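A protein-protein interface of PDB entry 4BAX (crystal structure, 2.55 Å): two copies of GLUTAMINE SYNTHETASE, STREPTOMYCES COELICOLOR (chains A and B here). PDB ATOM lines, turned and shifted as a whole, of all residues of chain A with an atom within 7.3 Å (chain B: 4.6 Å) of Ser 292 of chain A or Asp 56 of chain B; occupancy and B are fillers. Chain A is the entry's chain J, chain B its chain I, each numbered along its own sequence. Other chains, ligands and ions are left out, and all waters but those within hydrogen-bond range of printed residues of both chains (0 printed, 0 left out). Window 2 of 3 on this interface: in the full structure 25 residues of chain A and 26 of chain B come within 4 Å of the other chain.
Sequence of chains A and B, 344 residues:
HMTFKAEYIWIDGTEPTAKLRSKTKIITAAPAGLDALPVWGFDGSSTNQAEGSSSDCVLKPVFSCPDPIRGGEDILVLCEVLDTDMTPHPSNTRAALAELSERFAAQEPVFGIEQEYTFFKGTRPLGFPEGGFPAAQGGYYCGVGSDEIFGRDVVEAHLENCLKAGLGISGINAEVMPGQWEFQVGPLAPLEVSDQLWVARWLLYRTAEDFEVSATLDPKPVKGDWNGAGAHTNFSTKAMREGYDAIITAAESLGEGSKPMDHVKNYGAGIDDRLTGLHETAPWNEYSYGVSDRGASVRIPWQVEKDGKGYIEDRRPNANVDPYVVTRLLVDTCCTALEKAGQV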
ATOM      1  N   GLY A 290       0.702  -7.845  -0.721  1.00  0.00           N
ATOM      2  CA  GLY A 290       0.305  -8.532   0.484  1.00  0.00           C
ATOM      3  C   GLY A 290       0.863  -9.929   0.603  1.00  0.00           C
ATOM      4  O   GLY A 290       1.296 -10.548  -0.373  1.00  0.00           O
ATOM      5  N   VAL A 291       0.833 -10.423   1.833  1.00  0.00           N
ATOM      6  CA  VAL A 291       1.305 -11.755   2.145  1.00  0.00           C
ATOM      7  C   VAL A 291       0.226 -12.760   1.799  1.00  0.00           C
ATOM      8  O   VAL A 291      -0.906 -12.661   2.290  1.00  0.00           O
ATOM      9  CB  VAL A 291       1.669 -11.884   3.633  1.00  0.00           C
ATOM     10  CG1 VAL A 291       1.795 -13.343   4.023  1.00  0.00           C
ATOM     11  CG2 VAL A 291       2.950 -11.121   3.934  1.00  0.00           C
ATOM     12  N   SER A 292       0.572 -13.700   0.922  1.00  0.00           N
ATOM     13  CA  SER A 292      -0.321 -14.788   0.540  1.00  0.00           C
ATOM     14  C   SER A 292      -1.543 -14.245  -0.201  1.00  0.00           C
ATOM     15  O   SER A 292      -2.576 -14.915  -0.278  1.00  0.00           O
ATOM     16  CB  SER A 292      -0.744 -15.612   1.767  1.00  0.00           C
ATOM     17  OG  SER A 292      -0.061 -16.853   1.814  1.00  0.00           O
ATOM     18  N   ASP A 293      -1.429 -13.028  -0.736  1.00  0.00           N
ATOM     19  CA  ASP A 293      -2.561 -12.391  -1.396  1.00  0.00           C
ATOM     20  C   ASP A 293      -2.480 -12.602  -2.909  1.00  0.00           C
ATOM     21  O   ASP A 293      -1.684 -11.961  -3.589  1.00  0.00           O
ATOM     22  CB  ASP A 293      -2.580 -10.889  -1.085  1.00  0.00           C
ATOM     23  CG  ASP A 293      -3.868 -10.204  -1.539  1.00  0.00           C
ATOM     24  OD1 ASP A 293      -4.741 -10.873  -2.141  1.00  0.00           O
ATOM     25  OD2 ASP A 293      -3.993  -8.978  -1.326  1.00  0.00           O
ATOM     26  N   ARG A 294      -3.310 -13.488  -3.444  1.00  0.00           N
ATOM     27  CA  ARG A 294      -3.276 -13.727  -4.876  1.00  0.00           C
ATOM     28  C   ARG A 294      -4.002 -12.597  -5.625  1.00  0.00           C
ATOM     29  O   ARG A 294      -3.932 -12.524  -6.857  1.00  0.00           O
ATOM     30  CB  ARG A 294      -3.866 -15.094  -5.234  1.00  0.00           C
ATOM     31  CG  ARG A 294      -3.024 -16.302  -4.797  1.00  0.00           C
ATOM     32  CD  ARG A 294      -3.696 -17.618  -5.239  1.00  0.00           C
ATOM     33  NE  ARG A 294      -3.890 -18.637  -4.205  1.00  0.00           N
ATOM     34  CZ  ARG A 294      -4.768 -18.572  -3.205  1.00  0.00           C
ATOM     35  NH1 ARG A 294      -5.580 -17.529  -3.064  1.00  0.00           N
ATOM     36  NH2 ARG A 294      -4.836 -19.574  -2.341  1.00  0.00           N
ATOM     37  N   GLY A 295      -4.725 -11.749  -4.884  1.00  0.00           N
ATOM     38  CA  GLY A 295      -5.415 -10.604  -5.467  1.00  0.00           C
ATOM     39  C   GLY A 295      -4.583  -9.329  -5.512  1.00  0.00           C
ATOM     40  O   GLY A 295      -4.973  -8.345  -6.145  1.00  0.00           O
ATOM     41  N   ALA A 296      -3.440  -9.344  -4.833  1.00  0.00           N
ATOM     42  CA  ALA A 296      -2.518  -8.211  -4.822  1.00  0.00           C
ATOM     43  C   ALA A 296      -1.711  -8.113  -6.124  1.00  0.00           C
ATOM     44  O   ALA A 296      -1.569  -9.097  -6.837  1.00  0.00           O
ATOM     45  CB  ALA A 296      -1.595  -8.282  -3.603  1.00  0.00           C
ATOM     46  N   VAL A 298       1.544  -7.461  -6.154  1.00  0.00           N
ATOM     47  CA  VAL A 298       2.743  -8.206  -5.801  1.00  0.00           C
ATOM     48  C   VAL A 298       2.448  -9.075  -4.572  1.00  0.00           C
ATOM     49  O   VAL A 298       1.884  -8.600  -3.585  1.00  0.00           O
ATOM     50  CB  VAL A 298       3.926  -7.244  -5.502  1.00  0.00           C
ATOM     51  CG1 VAL A 298       5.041  -7.958  -4.727  1.00  0.00           C
ATOM     52  CG2 VAL A 298       4.472  -6.670  -6.807  1.00  0.00           C
ATOM     53  N   ARG A 299       2.841 -10.342  -4.620  1.00  0.00           N
ATOM     54  CA  ARG A 299       2.609 -11.244  -3.488  1.00  0.00           C
ATOM     55  C   ARG A 299       3.884 -11.608  -2.747  1.00  0.00           C
ATOM     56  O   ARG A 299       4.912 -11.887  -3.352  1.00  0.00           O
ATOM     57  CB  ARG A 299       1.912 -12.526  -3.951  1.00  0.00           C
ATOM     58  CG  ARG A 299       1.848 -13.627  -2.883  1.00  0.00           C
ATOM     59  CD  ARG A 299       1.035 -14.815  -3.362  1.00  0.00           C
ATOM     60  NE  ARG A 299       1.832 -15.666  -4.238  1.00  0.00           N
ATOM     61  CZ  ARG A 299       1.574 -16.948  -4.480  1.00  0.00           C
ATOM     62  NH1 ARG A 299       0.517 -17.539  -3.928  1.00  0.00           N
ATOM     63  NH2 ARG A 299       2.360 -17.633  -5.300  1.00  0.00           N
ATOM     64  N   ILE A 300       3.796 -11.613  -1.422  1.00  0.00           N
ATOM     65  CA  ILE A 300       4.843 -12.174  -0.597  1.00  0.00           C
ATOM     66  C   ILE A 300       4.402 -13.548  -0.122  1.00  0.00           C
ATOM     67  O   ILE A 300       3.443 -13.671   0.644  1.00  0.00           O
ATOM     68  CB  ILE A 300       5.120 -11.313   0.632  1.00  0.00           C
ATOM     69  CG1 ILE A 300       5.672  -9.942   0.233  1.00  0.00           C
ATOM     70  CG2 ILE A 300       6.078 -12.036   1.582  1.00  0.00           C
ATOM     71  CD1 ILE A 300       5.352  -8.856   1.227  1.00  0.00           C
ATOM     72  N   PRO A 301       5.092 -14.595  -0.593  1.00  0.00           N
ATOM     73  CA  PRO A 301       4.703 -15.966  -0.243  1.00  0.00           C
ATOM     74  C   PRO A 301       4.786 -16.196   1.270  1.00  0.00           C
ATOM     75  O   PRO A 301       5.618 -15.612   1.980  1.00  0.00           O
ATOM     76  CB  PRO A 301       5.744 -16.819  -0.978  1.00  0.00           C
ATOM     77  CG  PRO A 301       6.252 -15.925  -2.089  1.00  0.00           C
ATOM     78  CD  PRO A 301       6.261 -14.558  -1.489  1.00  0.00           C
ATOM     79  N   TRP A 302       3.927 -17.078   1.750  1.00  0.00           N
ATOM     80  CA  TRP A 302       3.811 -17.320   3.170  1.00  0.00           C
ATOM     81  C   TRP A 302       5.120 -17.849   3.753  1.00  0.00           C
ATOM     82  O   TRP A 302       5.468 -17.526   4.888  1.00  0.00           O
ATOM     83  CB  TRP A 302       2.632 -18.252   3.458  1.00  0.00           C
ATOM     84  CG  TRP A 302       2.826 -19.619   2.879  1.00  0.00           C
ATOM     85  CD1 TRP A 302       2.483 -20.034   1.614  1.00  0.00           C
ATOM     86  CD2 TRP A 302       3.378 -20.767   3.541  1.00  0.00           C
ATOM     87  NE1 TRP A 302       2.812 -21.364   1.447  1.00  0.00           N
ATOM     88  CE2 TRP A 302       3.357 -21.838   2.614  1.00  0.00           C
ATOM     89  CE3 TRP A 302       3.895 -20.995   4.822  1.00  0.00           C
ATOM     90  CZ2 TRP A 302       3.831 -23.114   2.931  1.00  0.00           C
ATOM     91  CZ3 TRP A 302       4.370 -22.268   5.133  1.00  0.00           C
ATOM     92  CH2 TRP A 302       4.334 -23.309   4.189  1.00  0.00           C
ATOM     93  N   GLN A 303       5.862 -18.629   2.971  1.00  0.00           N
ATOM     94  CA  GLN A 303       7.149 -19.155   3.435  1.00  0.00           C
ATOM     95  C   GLN A 303       8.162 -18.023   3.651  1.00  0.00           C
ATOM     96  O   GLN A 303       8.952 -18.047   4.593  1.00  0.00           O
ATOM     97  CB  GLN A 303       7.736 -20.138   2.415  1.00  0.00           C
ATOM     98  CG  GLN A 303       6.853 -21.315   2.037  1.00  0.00           C
ATOM     99  CD  GLN A 303       6.091 -21.058   0.746  1.00  0.00           C
ATOM    100  OE1 GLN A 303       5.758 -19.914   0.427  1.00  0.00           O
ATOM    101  NE2 GLN A 303       5.834 -22.122  -0.018  1.00  0.00           N
ATOM    102  N   GLU A 305       7.590 -14.825   4.403  1.00  0.00           N
ATOM    103  CA  GLU A 305       7.260 -14.058   5.589  1.00  0.00           C
ATOM    104  C   GLU A 305       7.579 -14.843   6.865  1.00  0.00           C
ATOM    105  O   GLU A 305       8.024 -14.264   7.861  1.00  0.00           O
ATOM    106  CB  GLU A 305       5.801 -13.605   5.534  1.00  0.00           C
ATOM    107  CG  GLU A 305       5.352 -12.725   6.679  1.00  0.00           C
ATOM    108  CD  GLU A 305       4.736 -13.518   7.806  1.00  0.00           C
ATOM    109  OE1 GLU A 305       3.919 -14.420   7.516  1.00  0.00           O
ATOM    110  OE2 GLU A 305       5.062 -13.236   8.978  1.00  0.00           O
ATOM    111  N   PHE B  42       1.107 -25.701  -3.812  1.00  0.00           N
ATOM    112  CA  PHE B  42       0.319 -25.274  -4.944  1.00  0.00           C
ATOM    113  C   PHE B  42      -0.784 -24.345  -4.477  1.00  0.00           C
ATOM    114  O   PHE B  42      -1.012 -24.193  -3.273  1.00  0.00           O
ATOM    115  CB  PHE B  42      -0.248 -26.479  -5.696  1.00  0.00           C
ATOM    116  CG  PHE B  42      -1.214 -27.280  -4.883  1.00  0.00           C
ATOM    117  CD1 PHE B  42      -0.753 -28.286  -4.037  1.00  0.00           C
ATOM    118  CD2 PHE B  42      -2.575 -27.021  -4.929  1.00  0.00           C
ATOM    119  CE1 PHE B  42      -1.636 -29.030  -3.265  1.00  0.00           C
ATOM    120  CE2 PHE B  42      -3.461 -27.759  -4.155  1.00  0.00           C
ATOM    121  CZ  PHE B  42      -2.991 -28.762  -3.326  1.00  0.00           C
ATOM    122  N   ASP B  43      -1.452 -23.719  -5.436  1.00  0.00           N
ATOM    123  CA  ASP B  43      -2.600 -22.862  -5.162  1.00  0.00           C
ATOM    124  C   ASP B  43      -3.915 -23.658  -5.219  1.00  0.00           C
ATOM    125  O   ASP B  43      -4.353 -24.116  -6.286  1.00  0.00           O
ATOM    126  CB  ASP B  43      -2.574 -21.645  -6.079  1.00  0.00           C
ATOM    127  CG  ASP B  43      -1.277 -20.809  -5.883  1.00  0.00           C
ATOM    128  OD1 ASP B  43      -0.641 -20.935  -4.810  1.00  0.00           O
ATOM    129  OD2 ASP B  43      -0.875 -20.035  -6.779  1.00  0.00           O
ATOM    130  N   SER B  54      -8.396 -17.693   0.179  1.00  0.00           N
ATOM    131  CA  SER B  54      -7.462 -17.948   1.303  1.00  0.00           C
ATOM    132  C   SER B  54      -6.592 -19.239   1.407  1.00  0.00           C
ATOM    133  O   SER B  54      -5.816 -19.375   2.355  1.00  0.00           O
ATOM    134  CB  SER B  54      -8.238 -17.784   2.624  1.00  0.00           C
ATOM    135  OG  SER B  54      -9.370 -18.641   2.659  1.00  0.00           O
ATOM    136  N   SER B  55      -6.660 -20.155   0.442  1.00  0.00           N
ATOM    137  CA  SER B  55      -5.925 -21.433   0.576  1.00  0.00           C
ATOM    138  C   SER B  55      -4.617 -21.720  -0.211  1.00  0.00           C
ATOM    139  O   SER B  55      -4.583 -21.785  -1.452  1.00  0.00           O
ATOM    140  CB  SER B  55      -6.895 -22.614   0.424  1.00  0.00           C
ATOM    141  OG  SER B  55      -6.359 -23.817   0.951  1.00  0.00           O
ATOM    142  N   ASP B  56      -3.553 -21.942   0.560  1.00  0.00           N
ATOM    143  CA  ASP B  56      -2.278 -22.331   0.006  1.00  0.00           C
ATOM    144  C   ASP B  56      -1.972 -23.683   0.607  1.00  0.00           C
ATOM    145  O   ASP B  56      -2.188 -23.908   1.797  1.00  0.00           O
ATOM    146  CB  ASP B  56      -1.228 -21.371   0.540  1.00  0.00           C
ATOM    147  CG  ASP B  56      -1.412 -19.976   0.023  1.00  0.00           C
ATOM    148  OD1 ASP B  56      -1.970 -19.818  -1.083  1.00  0.00           O
ATOM    149  OD2 ASP B  56      -1.038 -19.033   0.752  1.00  0.00           O
ATOM    150  N   CYS B  57      -1.461 -24.586  -0.221  1.00  0.00           N
ATOM    151  CA  CYS B  57      -1.344 -25.981   0.178  1.00  0.00           C
ATOM    152  C   CYS B  57       0.087 -26.494   0.082  1.00  0.00           C
ATOM    153  O   CYS B  57       0.926 -25.915  -0.595  1.00  0.00           O
ATOM    154  CB  CYS B  57      -2.274 -26.844  -0.677  1.00  0.00           C
ATOM    155  SG  CYS B  57      -4.048 -26.449  -0.548  1.00  0.00           S
ATOM    156  N   VAL B  58       0.360 -27.557   0.822  1.00  0.00           N
ATOM    157  CA  VAL B  58       1.686 -28.145   0.885  1.00  0.00           C
ATOM    158  C   VAL B  58       1.620 -29.564   0.335  1.00  0.00           C
ATOM    159  O   VAL B  58       0.677 -30.300   0.621  1.00  0.00           O
ATOM    160  CB  VAL B  58       2.210 -28.181   2.337  1.00  0.00           C
ATOM    161  CG1 VAL B  58       3.423 -29.115   2.459  1.00  0.00           C
ATOM    162  CG2 VAL B  58       2.532 -26.774   2.833  1.00  0.00           C
ATOM    163  N   THR B  84      -0.423 -25.242   5.641  1.00  0.00           N
ATOM    164  CA  THR B  84       0.889 -24.638   5.841  1.00  0.00           C
ATOM    165  C   THR B  84       1.483 -24.969   7.205  1.00  0.00           C
ATOM    166  O   THR B  84       2.702 -24.910   7.387  1.00  0.00           O
ATOM    167  CB  THR B  84       0.838 -23.114   5.661  1.00  0.00           C
ATOM    168  OG1 THR B  84      -0.145 -22.576   6.552  1.00  0.00           O
ATOM    169  CG2 THR B  84       0.491 -22.738   4.204  1.00  0.00           C
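The side-chain carboxylate (OD1) of Asp 43 of chain B is in salt-bridge range of the guanidinium group (NH1) of Arg 299 of chain A (3.7 Å).
OG of Ser 292 of chain A lies within hydrogen-bond range of OD2 of Asp 56 of chain B, at 2.6 Å.
The side-chain carboxylate (OD1) of Asp 56 of chain B is in salt-bridge range of the guanidinium group (NH2) of Arg 294 of chain A, 3.1 Å away.
NH2 of Arg 294 of chain A lies close to O of Ser 55 of chain B (2.4 Å).
Ser 292 of chain A touches just one residue of chain B: Asp 56.
Asp 56 of chain B touches three residues of chain A.
Printed residues of chain B within 4 Å of Arg 299 of chain A: Asp 43.
Of the printed residues of chain A, Val 58 of chain B touches Trp 302.
Among the printed residues, pairs that only touch across the chains: Arg 294 of chain A with Asp 43 of chain B (3.8 Å), Trp 302 of chain A with Asp 56 of chain B (3.8 Å), Trp 302 of chain A with Val 58 of chain B (3.9 Å) and Trp 302 of chain A with Thr 84 of chain B (3.4 Å).
N of Ser 292 of chain A is in hydrogen-bond range of O of Ile 300 of chain A (2.9 Å).
NE1 of Trp 302 of chain A lies close to OE1 of Gln 303 of chain A.
Of the 8 printed residues of chain B, 5 touch a printed residue of chain A.
Hydrophobic or aromatic side chains of chain B that line the printed part of chain A: Val 58.
Along chain B the printed residues that touch a printed residue of chain A span positions 43 to 84.
Of the 14 printed residues of chain A, 4 touch a printed residue of chain B.
Hydrophobic or aromatic side chains of chain A that line the printed part of chain B: Trp 302.
Among the printed residues, 8 pairs touch across the chains.
Among the printed residues, Asp or Glu carboxylates within 4 Å of a Lys or Arg side-chain nitrogen of the other chain: Arg 294 of chain A with Asp 56 of chain B and Arg 299 of chain A with Asp 43 of chain B.
No position is printed for both chains.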
